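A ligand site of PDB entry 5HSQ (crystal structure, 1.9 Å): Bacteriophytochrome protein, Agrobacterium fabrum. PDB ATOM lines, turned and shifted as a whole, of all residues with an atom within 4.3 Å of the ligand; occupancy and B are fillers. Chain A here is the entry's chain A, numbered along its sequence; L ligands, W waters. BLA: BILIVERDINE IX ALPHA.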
ATOM      1  N   CYS A  11       3.310   8.668  14.004  1.00  0.00           N
ATOM      2  CA  CYS A  11       3.908   8.341  12.673  1.00  0.00           C
ATOM      3  C   CYS A  11       4.255   9.575  11.839  1.00  0.00           C
ATOM      4  O   CYS A  11       5.372   9.636  11.150  1.00  0.00           O
ATOM      5  CB  CYS A  11       2.939   7.505  11.865  1.00  0.00           C
ATOM      6  SG  CYS A  11       2.732   5.872  12.606  1.00  0.00           S
ATOM      7  N   GLU A  14       7.596  11.997  12.892  1.00  0.00           N
ATOM      8  CA  GLU A  14       9.005  11.698  12.638  1.00  0.00           C
ATOM      9  C   GLU A  14       9.605  12.706  11.629  1.00  0.00           C
ATOM     10  O   GLU A  14       9.052  12.888  10.516  1.00  0.00           O
ATOM     11  CB  GLU A  14       9.187  10.264  12.147  1.00  0.00           C
ATOM     12  CG  GLU A  14      10.645   9.944  11.812  1.00  0.00           C
ATOM     13  CD  GLU A  14      10.796   8.574  11.220  1.00  0.00           C
ATOM     14  OE1 GLU A  14       9.727   7.884  10.895  1.00  0.00           O
ATOM     15  OE2 GLU A  14      11.964   8.209  11.063  1.00  0.00           O
ATOM     16  N   ILE A  16      11.490  13.026   9.032  1.00  0.00           N
ATOM     17  CA  ILE A  16      12.130  12.183   8.039  1.00  0.00           C
ATOM     18  C   ILE A  16      13.169  12.904   7.145  1.00  0.00           C
ATOM     19  O   ILE A  16      14.083  12.251   6.597  1.00  0.00           O
ATOM     20  CB  ILE A  16      11.125  11.413   7.165  1.00  0.00           C
ATOM     21  CG1 ILE A  16      10.298  12.321   6.229  1.00  0.00           C
ATOM     22  CG2 ILE A  16      10.242  10.478   8.069  1.00  0.00           C
ATOM     23  CD1 ILE A  16       9.473  11.592   5.181  1.00  0.00           C
ATOM     24  N   LEU A 155       3.851  -1.027  -9.713  1.00  0.00           N
ATOM     25  CA  LEU A 155       2.443  -0.747  -9.673  1.00  0.00           C
ATOM     26  C   LEU A 155       2.159   0.754  -9.653  1.00  0.00           C
ATOM     27  O   LEU A 155       3.058   1.615  -9.408  1.00  0.00           O
ATOM     28  CB  LEU A 155       1.786  -1.531  -8.524  1.00  0.00           C
ATOM     29  CG  LEU A 155       2.228  -1.186  -7.127  1.00  0.00           C
ATOM     30  CD1 LEU A 155       1.531   0.125  -6.653  1.00  0.00           C
ATOM     31  CD2 LEU A 155       1.882  -2.304  -6.154  1.00  0.00           C
ATOM     32  N   TYR A 157      -0.388   3.398  -7.868  1.00  0.00           N
ATOM     33  CA  TYR A 157      -1.113   3.527  -6.616  1.00  0.00           C
ATOM     34  C   TYR A 157      -1.844   4.874  -6.681  1.00  0.00           C
ATOM     35  O   TYR A 157      -1.218   5.901  -6.755  1.00  0.00           O
ATOM     36  CB  TYR A 157      -0.139   3.465  -5.449  1.00  0.00           C
ATOM     37  CG  TYR A 157      -0.748   3.444  -4.067  1.00  0.00           C
ATOM     38  CD1 TYR A 157      -1.613   2.400  -3.652  1.00  0.00           C
ATOM     39  CD2 TYR A 157      -0.498   4.493  -3.134  1.00  0.00           C
ATOM     40  CE1 TYR A 157      -2.138   2.378  -2.371  1.00  0.00           C
ATOM     41  CE2 TYR A 157      -1.040   4.461  -1.843  1.00  0.00           C
ATOM     42  CZ  TYR A 157      -1.811   3.390  -1.486  1.00  0.00           C
ATOM     43  OH  TYR A 157      -2.404   3.353  -0.248  1.00  0.00           O
ATOM     44  N   TYR A 179      -0.890  -7.198  -5.993  1.00  0.00           N
ATOM     45  CA  TYR A 179      -1.766  -6.374  -5.214  1.00  0.00           C
ATOM     46  C   TYR A 179      -2.777  -5.609  -6.033  1.00  0.00           C
ATOM     47  O   TYR A 179      -3.493  -4.757  -5.487  1.00  0.00           O
ATOM     48  CB  TYR A 179      -0.987  -5.385  -4.395  1.00  0.00           C
ATOM     49  CG  TYR A 179      -0.055  -5.973  -3.330  1.00  0.00           C
ATOM     50  CD1 TYR A 179      -0.408  -7.131  -2.588  1.00  0.00           C
ATOM     51  CD2 TYR A 179       1.154  -5.338  -3.041  1.00  0.00           C
ATOM     52  CE1 TYR A 179       0.452  -7.636  -1.615  1.00  0.00           C
ATOM     53  CE2 TYR A 179       1.972  -5.813  -2.038  1.00  0.00           C
ATOM     54  CZ  TYR A 179       1.614  -6.942  -1.328  1.00  0.00           C
ATOM     55  OH  TYR A 179       2.514  -7.367  -0.404  1.00  0.00           O
ATOM     56  N   PHE A 184      -5.049   0.167   0.383  1.00  0.00           N
ATOM     57  CA  PHE A 184      -4.095   0.222   1.475  1.00  0.00           C
ATOM     58  C   PHE A 184      -4.439   1.490   2.253  1.00  0.00           C
ATOM     59  O   PHE A 184      -4.891   2.489   1.670  1.00  0.00           O
ATOM     60  CB  PHE A 184      -2.661   0.284   0.960  1.00  0.00           C
ATOM     61  CG  PHE A 184      -2.142  -1.008   0.385  1.00  0.00           C
ATOM     62  CD1 PHE A 184      -2.607  -1.447  -0.824  1.00  0.00           C
ATOM     63  CD2 PHE A 184      -1.184  -1.752   1.039  1.00  0.00           C
ATOM     64  CE1 PHE A 184      -2.162  -2.641  -1.343  1.00  0.00           C
ATOM     65  CE2 PHE A 184      -0.753  -2.935   0.538  1.00  0.00           C
ATOM     66  CZ  PHE A 184      -1.245  -3.364  -0.636  1.00  0.00           C
ATOM     67  N   GLY A 187      -2.495   5.542   6.532  1.00  0.00           N
ATOM     68  CA  GLY A 187      -1.332   5.538   7.416  1.00  0.00           C
ATOM     69  C   GLY A 187      -0.060   4.783   6.923  1.00  0.00           C
ATOM     70  O   GLY A 187       1.019   5.011   7.442  1.00  0.00           O
ATOM     71  N   ASP A 188      -0.155   4.034   5.845  1.00  0.00           N
ATOM     72  CA  ASP A 188       1.036   3.430   5.205  1.00  0.00           C
ATOM     73  C   ASP A 188       1.983   4.481   4.644  1.00  0.00           C
ATOM     74  O   ASP A 188       3.189   4.166   4.475  1.00  0.00           O
ATOM     75  CB  ASP A 188       0.666   2.456   4.046  1.00  0.00           C
ATOM     76  CG  ASP A 188       0.033   1.144   4.504  1.00  0.00           C
ATOM     77  OD1 ASP A 188      -0.396   1.010   5.641  1.00  0.00           O
ATOM     78  OD2 ASP A 188      -0.094   0.204   3.681  1.00  0.00           O
ATOM     79  N   ILE A 189       1.451   5.644   4.262  1.00  0.00           N
ATOM     80  CA  ILE A 189       2.267   6.806   3.865  1.00  0.00           C
ATOM     81  C   ILE A 189       1.841   8.002   4.679  1.00  0.00           C
ATOM     82  O   ILE A 189       0.932   8.680   4.331  1.00  0.00           O
ATOM     83  CB  ILE A 189       2.228   7.135   2.339  1.00  0.00           C
ATOM     84  CG1 ILE A 189       2.331   5.846   1.552  1.00  0.00           C
ATOM     85  CG2 ILE A 189       3.351   8.141   1.983  1.00  0.00           C
ATOM     86  CD1 ILE A 189       2.243   5.982   0.053  1.00  0.00           C
ATOM     87  N   PRO A 190       2.505   8.256   5.807  1.00  0.00           N
ATOM     88  CA  PRO A 190       2.062   9.363   6.670  1.00  0.00           C
ATOM     89  C   PRO A 190       2.178  10.766   6.047  1.00  0.00           C
ATOM     90  O   PRO A 190       2.909  10.929   5.056  1.00  0.00           O
ATOM     91  CB  PRO A 190       2.842   9.168   7.958  1.00  0.00           C
ATOM     92  CG  PRO A 190       3.965   8.312   7.606  1.00  0.00           C
ATOM     93  CD  PRO A 190       3.644   7.527   6.354  1.00  0.00           C
ATOM     94  N   ALA A 193       5.457  12.418   4.921  1.00  0.00           N
ATOM     95  CA  ALA A 193       6.008  11.705   3.785  1.00  0.00           C
ATOM     96  C   ALA A 193       5.230  12.152   2.536  1.00  0.00           C
ATOM     97  O   ALA A 193       5.853  12.531   1.543  1.00  0.00           O
ATOM     98  CB  ALA A 193       5.982  10.210   3.994  1.00  0.00           C
ATOM     99  N   TYR A 197       6.886  14.002  -0.625  1.00  0.00           N
ATOM    100  CA  TYR A 197       6.769  13.345  -1.912  1.00  0.00           C
ATOM    101  C   TYR A 197       6.042  14.194  -2.941  1.00  0.00           C
ATOM    102  O   TYR A 197       6.098  13.919  -4.118  1.00  0.00           O
ATOM    103  CB  TYR A 197       6.134  11.942  -1.742  1.00  0.00           C
ATOM    104  CG  TYR A 197       6.917  10.977  -0.915  1.00  0.00           C
ATOM    105  CD1 TYR A 197       8.182  11.242  -0.428  1.00  0.00           C
ATOM    106  CD2 TYR A 197       6.325   9.826  -0.500  1.00  0.00           C
ATOM    107  CE1 TYR A 197       8.836  10.342   0.394  1.00  0.00           C
ATOM    108  CE2 TYR A 197       6.952   8.924   0.314  1.00  0.00           C
ATOM    109  CZ  TYR A 197       8.231   9.146   0.717  1.00  0.00           C
ATOM    110  OH  TYR A 197       8.845   8.223   1.505  1.00  0.00           O
ATOM    111  N   ARG A 203      12.301   8.640  -5.161  1.00  0.00           N
ATOM    112  CA  ARG A 203      13.004   7.952  -4.084  1.00  0.00           C
ATOM    113  C   ARG A 203      13.425   6.544  -4.441  1.00  0.00           C
ATOM    114  O   ARG A 203      12.828   5.893  -5.287  1.00  0.00           O
ATOM    115  CB  ARG A 203      12.189   8.019  -2.770  1.00  0.00           C
ATOM    116  CG  ARG A 203      10.842   7.245  -2.854  1.00  0.00           C
ATOM    117  CD  ARG A 203       9.754   7.988  -2.118  1.00  0.00           C
ATOM    118  NE  ARG A 203       9.432   9.272  -2.720  1.00  0.00           N
ATOM    119  CZ  ARG A 203       8.577   9.446  -3.719  1.00  0.00           C
ATOM    120  NH1 ARG A 203       8.399  10.670  -4.222  1.00  0.00           N
ATOM    121  NH2 ARG A 203       7.837   8.453  -4.185  1.00  0.00           N
ATOM    122  N   ILE A 205      15.425   2.929  -2.570  1.00  0.00           N
ATOM    123  CA  ILE A 205      15.939   2.185  -1.447  1.00  0.00           C
ATOM    124  C   ILE A 205      16.475   0.844  -1.993  1.00  0.00           C
ATOM    125  O   ILE A 205      15.719  -0.155  -2.101  1.00  0.00           O
ATOM    126  CB  ILE A 205      14.902   1.913  -0.335  1.00  0.00           C
ATOM    127  CG1 ILE A 205      14.277   3.228   0.168  1.00  0.00           C
ATOM    128  CG2 ILE A 205      15.575   1.148   0.830  1.00  0.00           C
ATOM    129  CD1 ILE A 205      12.924   3.069   0.919  1.00  0.00           C
ATOM    130  N   ARG A 235      19.286  10.072   1.000  1.00  0.00           N
ATOM    131  CA  ARG A 235      18.852  10.259   2.401  1.00  0.00           C
ATOM    132  C   ARG A 235      18.511   8.908   3.048  1.00  0.00           C
ATOM    133  O   ARG A 235      17.826   8.112   2.438  1.00  0.00           O
ATOM    134  CB  ARG A 235      17.580  11.103   2.357  1.00  0.00           C
ATOM    135  CG  ARG A 235      16.906  11.428   3.694  1.00  0.00           C
ATOM    136  CD  ARG A 235      15.678  12.309   3.523  1.00  0.00           C
ATOM    137  NE  ARG A 235      14.643  11.759   2.686  1.00  0.00           N
ATOM    138  CZ  ARG A 235      13.786  10.804   3.034  1.00  0.00           C
ATOM    139  NH1 ARG A 235      13.816  10.253   4.274  1.00  0.00           N
ATOM    140  NH2 ARG A 235      12.855  10.428   2.166  1.00  0.00           N
ATOM    141  N   VAL A 237      16.356   6.544   5.191  1.00  0.00           N
ATOM    142  CA  VAL A 237      14.898   6.575   5.295  1.00  0.00           C
ATOM    143  C   VAL A 237      14.420   6.118   6.669  1.00  0.00           C
ATOM    144  O   VAL A 237      15.140   5.519   7.438  1.00  0.00           O
ATOM    145  CB  VAL A 237      14.185   5.788   4.180  1.00  0.00           C
ATOM    146  CG1 VAL A 237      14.578   6.350   2.776  1.00  0.00           C
ATOM    147  CG2 VAL A 237      14.576   4.335   4.237  1.00  0.00           C
ATOM    148  N   SER A 238      13.143   6.443   6.920  1.00  0.00           N
ATOM    149  CA  SER A 238      12.529   6.085   8.189  1.00  0.00           C
ATOM    150  C   SER A 238      12.680   4.593   8.520  1.00  0.00           C
ATOM    151  O   SER A 238      12.348   3.745   7.719  1.00  0.00           O
ATOM    152  CB  SER A 238      11.074   6.471   8.145  1.00  0.00           C
ATOM    153  OG  SER A 238      10.451   5.858   9.300  1.00  0.00           O
ATOM    154  N   VAL A 240      10.864   2.775  10.407  1.00  0.00           N
ATOM    155  CA  VAL A 240       9.591   2.100  10.447  1.00  0.00           C
ATOM    156  C   VAL A 240       9.159   1.734   9.024  1.00  0.00           C
ATOM    157  O   VAL A 240       8.586   0.718   8.811  1.00  0.00           O
ATOM    158  CB  VAL A 240       8.546   2.928  11.269  1.00  0.00           C
ATOM    159  CG1 VAL A 240       8.195   4.216  10.547  1.00  0.00           C
ATOM    160  CG2 VAL A 240       7.282   2.130  11.493  1.00  0.00           C
ATOM    161  N   HIS A 241       9.508   2.551   8.022  1.00  0.00           N
ATOM    162  CA  HIS A 241       9.227   2.133   6.647  1.00  0.00           C
ATOM    163  C   HIS A 241      10.055   0.932   6.256  1.00  0.00           C
ATOM    164  O   HIS A 241       9.611   0.112   5.523  1.00  0.00           O
ATOM    165  CB  HIS A 241       9.477   3.265   5.621  1.00  0.00           C
ATOM    166  CG  HIS A 241       9.146   2.845   4.238  1.00  0.00           C
ATOM    167  ND1 HIS A 241       7.920   2.288   3.919  1.00  0.00           N
ATOM    168  CD2 HIS A 241       9.943   2.686   3.143  1.00  0.00           C
ATOM    169  CE1 HIS A 241       7.926   1.897   2.664  1.00  0.00           C
ATOM    170  NE2 HIS A 241       9.142   2.141   2.172  1.00  0.00           N
ATOM    171  N   TYR A 244       8.317  -1.962   7.447  1.00  0.00           N
ATOM    172  CA  TYR A 244       7.174  -2.228   6.546  1.00  0.00           C
ATOM    173  C   TYR A 244       7.651  -3.028   5.308  1.00  0.00           C
ATOM    174  O   TYR A 244       7.040  -4.003   4.897  1.00  0.00           O
ATOM    175  CB  TYR A 244       6.536  -0.911   6.119  1.00  0.00           C
ATOM    176  CG  TYR A 244       5.355  -0.931   5.155  1.00  0.00           C
ATOM    177  CD1 TYR A 244       5.531  -1.069   3.761  1.00  0.00           C
ATOM    178  CD2 TYR A 244       4.039  -0.740   5.604  1.00  0.00           C
ATOM    179  CE1 TYR A 244       4.467  -1.071   2.870  1.00  0.00           C
ATOM    180  CE2 TYR A 244       2.981  -0.692   4.707  1.00  0.00           C
ATOM    181  CZ  TYR A 244       3.178  -0.858   3.350  1.00  0.00           C
ATOM    182  OH  TYR A 244       2.112  -0.786   2.546  1.00  0.00           O
ATOM    183  N   MET A 245       8.786  -2.601   4.734  1.00  0.00           N
ATOM    184  CA  MET A 245       9.339  -3.283   3.584  1.00  0.00           C
ATOM    185  C   MET A 245       9.664  -4.748   3.924  1.00  0.00           C
ATOM    186  O   MET A 245       9.348  -5.633   3.173  1.00  0.00           O
ATOM    187  CB  MET A 245      10.587  -2.559   3.045  1.00  0.00           C
ATOM    188  CG  MET A 245      10.267  -1.238   2.361  1.00  0.00           C
ATOM    189  SD  MET A 245      11.737  -0.363   1.821  1.00  0.00           S
ATOM    190  CE  MET A 245      12.300  -1.521   0.561  1.00  0.00           C
ATOM    191  N   MET A 248       6.620  -6.736   4.146  1.00  0.00           N
ATOM    192  CA  MET A 248       6.090  -6.972   2.822  1.00  0.00           C
ATOM    193  C   MET A 248       6.955  -7.978   2.016  1.00  0.00           C
ATOM    194  O   MET A 248       6.508  -8.517   1.051  1.00  0.00           O
ATOM    195  CB  MET A 248       5.978  -5.624   2.085  1.00  0.00           C
ATOM    196  CG  MET A 248       5.092  -5.661   0.866  1.00  0.00           C
ATOM    197  SD  MET A 248       4.773  -4.126   0.021  1.00  0.00           S
ATOM    198  CE  MET A 248       3.211  -3.625   0.726  1.00  0.00           C
ATOM    199  N   SER A 253      13.168  -0.948  -3.104  1.00  0.00           N
ATOM    200  CA  SER A 253      12.079  -0.216  -3.665  1.00  0.00           C
ATOM    201  C   SER A 253      12.571   1.008  -4.417  1.00  0.00           C
ATOM    202  O   SER A 253      13.734   1.414  -4.292  1.00  0.00           O
ATOM    203  CB  SER A 253      11.015   0.189  -2.638  1.00  0.00           C
ATOM    204  OG  SER A 253      11.516   1.129  -1.727  1.00  0.00           O
ATOM    205  N   MET A 254      11.665   1.537  -5.220  1.00  0.00           N
ATOM    206  CA  MET A 254      11.834   2.819  -5.919  1.00  0.00           C
ATOM    207  C   MET A 254      10.423   3.316  -6.220  1.00  0.00           C
ATOM    208  O   MET A 254       9.579   2.529  -6.701  1.00  0.00           O
ATOM    209  CB  MET A 254      12.625   2.681  -7.239  1.00  0.00           C
ATOM    210  CG  MET A 254      12.633   4.012  -8.027  1.00  0.00           C
ATOM    211  SD  MET A 254      13.413   3.833  -9.609  1.00  0.00           S
ATOM    212  CE  MET A 254      11.929   3.283 -10.483  1.00  0.00           C
ATOM    213  N   SER A 255      10.140   4.552  -5.822  1.00  0.00           N
ATOM    214  CA  SER A 255       8.895   5.144  -6.191  1.00  0.00           C
ATOM    215  C   SER A 255       8.994   6.560  -6.716  1.00  0.00           C
ATOM    216  O   SER A 255       9.975   7.230  -6.559  1.00  0.00           O
ATOM    217  CB  SER A 255       7.857   4.983  -5.052  1.00  0.00           C
ATOM    218  OG  SER A 255       8.299   5.640  -3.878  1.00  0.00           O
ATOM    219  N   LEU A 267       1.316   7.297  -6.923  1.00  0.00           N
ATOM    220  CA  LEU A 267       2.703   6.843  -7.031  1.00  0.00           C
ATOM    221  C   LEU A 267       2.793   5.763  -8.072  1.00  0.00           C
ATOM    222  O   LEU A 267       1.867   4.946  -8.216  1.00  0.00           O
ATOM    223  CB  LEU A 267       3.205   6.276  -5.710  1.00  0.00           C
ATOM    224  CG  LEU A 267       3.196   7.059  -4.398  1.00  0.00           C
ATOM    225  CD1 LEU A 267       3.882   6.292  -3.273  1.00  0.00           C
ATOM    226  CD2 LEU A 267       3.946   8.378  -4.568  1.00  0.00           C
ATOM    227  N   HIS A 271       9.158  -2.525  -6.606  1.00  0.00           N
ATOM    228  CA  HIS A 271       9.796  -3.368  -5.597  1.00  0.00           C
ATOM    229  C   HIS A 271      10.556  -4.551  -6.203  1.00  0.00           C
ATOM    230  O   HIS A 271      10.226  -5.060  -7.309  1.00  0.00           O
ATOM    231  CB  HIS A 271       8.751  -3.968  -4.664  1.00  0.00           C
ATOM    232  CG  HIS A 271       7.914  -2.935  -3.976  1.00  0.00           C
ATOM    233  ND1 HIS A 271       6.773  -2.467  -4.539  1.00  0.00           N
ATOM    234  CD2 HIS A 271       8.141  -2.200  -2.863  1.00  0.00           C
ATOM    235  CE1 HIS A 271       6.243  -1.546  -3.721  1.00  0.00           C
ATOM    236  NE2 HIS A 271       7.111  -1.319  -2.743  1.00  0.00           N
ATOM    237  N   THR A 443      -2.002  -1.713  13.237  1.00  0.00           N
ATOM    238  CA  THR A 443      -0.693  -1.191  13.582  1.00  0.00           C
ATOM    239  C   THR A 443      -0.513  -1.505  15.056  1.00  0.00           C
ATOM    240  O   THR A 443      -1.441  -1.335  15.812  1.00  0.00           O
ATOM    241  CB  THR A 443      -0.622   0.286  13.351  1.00  0.00           C
ATOM    242  OG1 THR A 443      -1.699   0.956  14.018  1.00  0.00           O
ATOM    243  CG2 THR A 443      -0.728   0.633  11.871  1.00  0.00           C
ATOM    244  N   ILE A 450       4.547   3.138  16.902  1.00  0.00           N
ATOM    245  CA  ILE A 450       3.549   2.470  16.087  1.00  0.00           C
ATOM    246  C   ILE A 450       4.271   1.647  14.993  1.00  0.00           C
ATOM    247  O   ILE A 450       5.073   2.201  14.178  1.00  0.00           O
ATOM    248  CB  ILE A 450       2.625   3.488  15.489  1.00  0.00           C
ATOM    249  CG1 ILE A 450       1.944   4.315  16.617  1.00  0.00           C
ATOM    250  CG2 ILE A 450       1.603   2.816  14.585  1.00  0.00           C
ATOM    251  CD1 ILE A 450       1.268   3.427  17.704  1.00  0.00           C
ATOM    252  N   HIS A 451       4.021   0.352  14.956  1.00  0.00           N
ATOM    253  CA  HIS A 451       4.667  -0.542  13.929  1.00  0.00           C
ATOM    254  C   HIS A 451       3.674  -1.018  12.873  1.00  0.00           C
ATOM    255  O   HIS A 451       2.450  -1.249  13.199  1.00  0.00           O
ATOM    256  CB  HIS A 451       5.282  -1.729  14.620  1.00  0.00           C
ATOM    257  CG  HIS A 451       6.283  -1.335  15.621  1.00  0.00           C
ATOM    258  ND1 HIS A 451       7.617  -1.179  15.310  1.00  0.00           N
ATOM    259  CD2 HIS A 451       6.132  -0.920  16.905  1.00  0.00           C
ATOM    260  CE1 HIS A 451       8.269  -0.767  16.379  1.00  0.00           C
ATOM    261  NE2 HIS A 451       7.386  -0.606  17.372  1.00  0.00           N
ATOM    262  N   PRO A 452       4.158  -1.277  11.631  1.00  0.00           N
ATOM    263  CA  PRO A 452       3.209  -1.709  10.618  1.00  0.00           C
ATOM    264  C   PRO A 452       2.779  -3.183  10.810  1.00  0.00           C
ATOM    265  O   PRO A 452       3.424  -3.961  11.426  1.00  0.00           O
ATOM    266  CB  PRO A 452       4.037  -1.565   9.295  1.00  0.00           C
ATOM    267  CG  PRO A 452       5.436  -1.748   9.717  1.00  0.00           C
ATOM    268  CD  PRO A 452       5.499  -1.051  11.053  1.00  0.00           C
HETATM  269  CHA BLA L   1       7.074   5.522   3.051  1.00  0.00           C
HETATM  270  NA  BLA L   1       5.241   3.911   2.346  1.00  0.00           N
HETATM  271  C1A BLA L   1       6.353   4.713   2.133  1.00  0.00           C
HETATM  272  C2A BLA L   1       6.661   4.552   0.774  1.00  0.00           C
HETATM  273  C3A BLA L   1       5.769   3.708   0.197  1.00  0.00           C
HETATM  274  C4A BLA L   1       4.851   3.328   1.208  1.00  0.00           C
HETATM  275  CMA BLA L   1       5.636   3.354  -1.259  1.00  0.00           C
HETATM  276  CAA BLA L   1       7.830   5.365   0.045  1.00  0.00           C
HETATM  277  CBA BLA L   1       9.105   4.560   0.051  1.00  0.00           C
HETATM  278  CGA BLA L   1       9.183   3.430  -0.992  1.00  0.00           C
HETATM  279  O1A BLA L   1       9.047   3.655  -2.235  1.00  0.00           O
HETATM  280  O2A BLA L   1       9.362   2.305  -0.506  1.00  0.00           O
HETATM  281  CHB BLA L   1       3.751   2.526   1.143  1.00  0.00           C
HETATM  282  NB  BLA L   1       4.353   0.701  -0.311  1.00  0.00           N
HETATM  283  C1B BLA L   1       3.454   1.546   0.253  1.00  0.00           C
HETATM  284  C2B BLA L   1       2.170   1.155  -0.103  1.00  0.00           C
HETATM  285  C3B BLA L   1       2.274   0.122  -0.985  1.00  0.00           C
HETATM  286  C4B BLA L   1       3.635  -0.112  -1.071  1.00  0.00           C
HETATM  287  CMB BLA L   1       0.825   1.803   0.310  1.00  0.00           C
HETATM  288  OB  BLA L   1       4.170  -0.997  -1.747  1.00  0.00           O
HETATM  289  CAB BLA L   1       1.174  -0.481  -1.582  1.00  0.00           C
HETATM  290  CBB BLA L   1       1.223  -1.617  -2.508  1.00  0.00           C
HETATM  291  NC  BLA L   1       4.252   3.218   7.414  1.00  0.00           N
HETATM  292  C1C BLA L   1       3.449   2.452   8.175  1.00  0.00           C
HETATM  293  C2C BLA L   1       3.360   2.999   9.430  1.00  0.00           C
HETATM  294  C3C BLA L   1       4.237   4.061   9.493  1.00  0.00           C
HETATM  295  C4C BLA L   1       4.777   4.174   8.199  1.00  0.00           C
HETATM  296  CMC BLA L   1       2.674   2.395  10.617  1.00  0.00           C
HETATM  297  OC  BLA L   1       2.779   1.482   7.716  1.00  0.00           O
HETATM  298  CAC BLA L   1       4.623   4.965  10.636  1.00  0.00           C
HETATM  299  CBC BLA L   1       4.123   4.729  12.042  1.00  0.00           C
HETATM  300  CHD BLA L   1       5.626   5.210   7.883  1.00  0.00           C
HETATM  301  ND  BLA L   1       6.089   5.090   5.355  1.00  0.00           N
HETATM  302  C1D BLA L   1       6.249   5.568   6.631  1.00  0.00           C
HETATM  303  C2D BLA L   1       7.190   6.557   6.530  1.00  0.00           C
HETATM  304  C3D BLA L   1       7.584   6.701   5.197  1.00  0.00           C
HETATM  305  C4D BLA L   1       6.902   5.771   4.458  1.00  0.00           C
HETATM  306  CMD BLA L   1       7.712   7.406   7.650  1.00  0.00           C
HETATM  307  CAD BLA L   1       8.607   7.600   4.753  1.00  0.00           C
HETATM  308  CBD BLA L   1       9.930   6.919   4.297  1.00  0.00           C
HETATM  309  CGD BLA L   1      11.088   7.979   3.988  1.00  0.00           C
HETATM  310  O1D BLA L   1      10.964   8.613   2.939  1.00  0.00           O
HETATM  311  O2D BLA L   1      11.935   8.231   4.863  1.00  0.00           O
HETATM  312  O   HOH W   1       0.063   1.175   8.272  1.00  0.00           O
HETATM  313  O   HOH W   2      12.002   3.766  -2.688  1.00  0.00           O
HETATM  314  O   HOH W   3       7.876   1.623  -3.914  1.00  0.00           O
HETATM  315  O   HOH W   4       5.480   2.277   5.081  1.00  0.00           O
HETATM  316  O   HOH W   5       7.354   0.307  -0.418  1.00  0.00           O
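SD of Met 248 sits close to OB of the ligand, 3.6 Å away.
Residues that only touch the ligand: Glu 14 (3.8 Å), Leu 155 (3.8 Å), Tyr 157 (3.6 Å), Tyr 179 (3.8 Å), Phe 184 (3.6 Å), Gly 187 (3.6 Å), Ile 189 (3.6 Å), Pro 190 (3.3 Å), Ala 193 (3.8 Å), Arg 203 (3.9 Å), Ile 205 (3.9 Å), Val 237 (3.4 Å), Val 240 (3.7 Å), Tyr 244 (3.3 Å), Leu 267 (3.97 Å), Ile 450 (3.4 Å) and Pro 452 (3.7 Å).
Hydrophobic or aromatic side chains within 4 Å of the ligand: Leu 155, Tyr 157, Tyr 179, Phe 184, Ile 189, Pro 190, Ala 193, Tyr 197, Ile 205, Val 237, Val 240, His 241, Tyr 244, Met 248, Leu 267, His 271, Ile 450 and Pro 452.
Within 4 Å of the ligand: Cys 11, Glu 14, Leu 155, Tyr 157, Tyr 179, Phe 184, Gly 187, Asp 188, Ile 189, Pro 190, Ala 193, Tyr 197, Arg 203, Ile 205, Arg 235, Val 237, Ser 238, Val 240, His 241, Tyr 244, Met 248, Ser 253, Ser 255, Leu 267, His 271, Ile 450 and Pro 452.
The nearest printed residue that does not touch the ligand is Ile 16 (4.002 Å).
NE2 of His 271 lies close to OB of the ligand (3.1 Å).
An oxygen (O2A) of the ligand lies within hydrogen-bond range of a ring nitrogen (NE2) of His 241, at 2.7 Å.
The side-chain hydroxyl of Tyr 197 is in hydrogen-bond range of an oxygen (O1D) of the ligand.
The guanidinium group of Arg 235 lies within salt-bridge range of an oxygen (O1D) of the ligand (2.7 Å).
The backbone carbonyl oxygen (O) of Asp 188 is in hydrogen-bond range of a nitrogen (NA) of the ligand (3.0 Å).
The side-chain hydroxyl (OG) of Ser 255 is in hydrogen-bond range of an oxygen (O1A) of the ligand, 2.7 Å away.
An oxygen (O2A) of the ligand lies within hydrogen-bond range of the side-chain hydroxyl (OG) of Ser 253, 2.7 Å away.
The side-chain sulfur (SG) of Cys 11 is bonded to a carbon (CBC) of the ligand, 1.9 Å away.
The backbone NH (N) of Ser 238 sits at hydrogen-bond distance from an oxygen (O2D) of the ligand (3.0 Å).
OD2 of Asp 188 sits at hydrogen-bond distance from OH of Tyr 244 (2.7 Å).
The side-chain hydroxyl of Tyr 157 lies within hydrogen-bond range of the backbone carbonyl oxygen of Phe 184, at 3.3 Å.
The backbone carbonyl oxygen of Ile 16 lies within hydrogen-bond range of the guanidinium group of Arg 235, 3.1 Å away.
The backbone NH of Val 240 lies close to the side-chain hydroxyl of Ser 238.
OG of Ser 238 sits at hydrogen-bond distance from OE1 of Glu 14 (2.7 Å).
The backbone NH (N) of Ile 205 is in hydrogen-bond range of the backbone carbonyl oxygen (O) of Ser 253, 2.8 Å away.
The side-chain sulfur (SD) of Met 245 lies close to a ring nitrogen (NE2) of His 241.
The backbone NH of Tyr 157 lies within hydrogen-bond range of the backbone carbonyl oxygen of Leu 267.
Water W1 bridges the side-chain carboxylate (OD1) of Asp 188 (2.7 Å) and an oxygen (OC) of the ligand (2.8 Å).
Water W4 lies within hydrogen-bond range of ND1 of His 241 (2.7 Å), NC of the ligand (2.8 Å) and O of Asp 188 (3.0 Å).
Water W5 lies within hydrogen-bond range of an oxygen (O2A) of the ligand (2.8 Å) and a ring nitrogen (NE2) of His 271 (2.8 Å).
Water W3 lies within hydrogen-bond range of an oxygen (O1A) of the ligand (2.9 Å), a ring nitrogen (NE2) of His 271 (3.3 Å) and the backbone carbonyl oxygen (O) of Met 254 (3.4 Å).
Water W2 lies within hydrogen-bond range of the side-chain hydroxyl of Ser 253 (2.8 Å), an oxygen (O1A) of the ligand (3.0 Å), the backbone NH of Met 254 (3.4 Å) and the backbone carbonyl oxygen of Arg 203 (3.5 Å).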
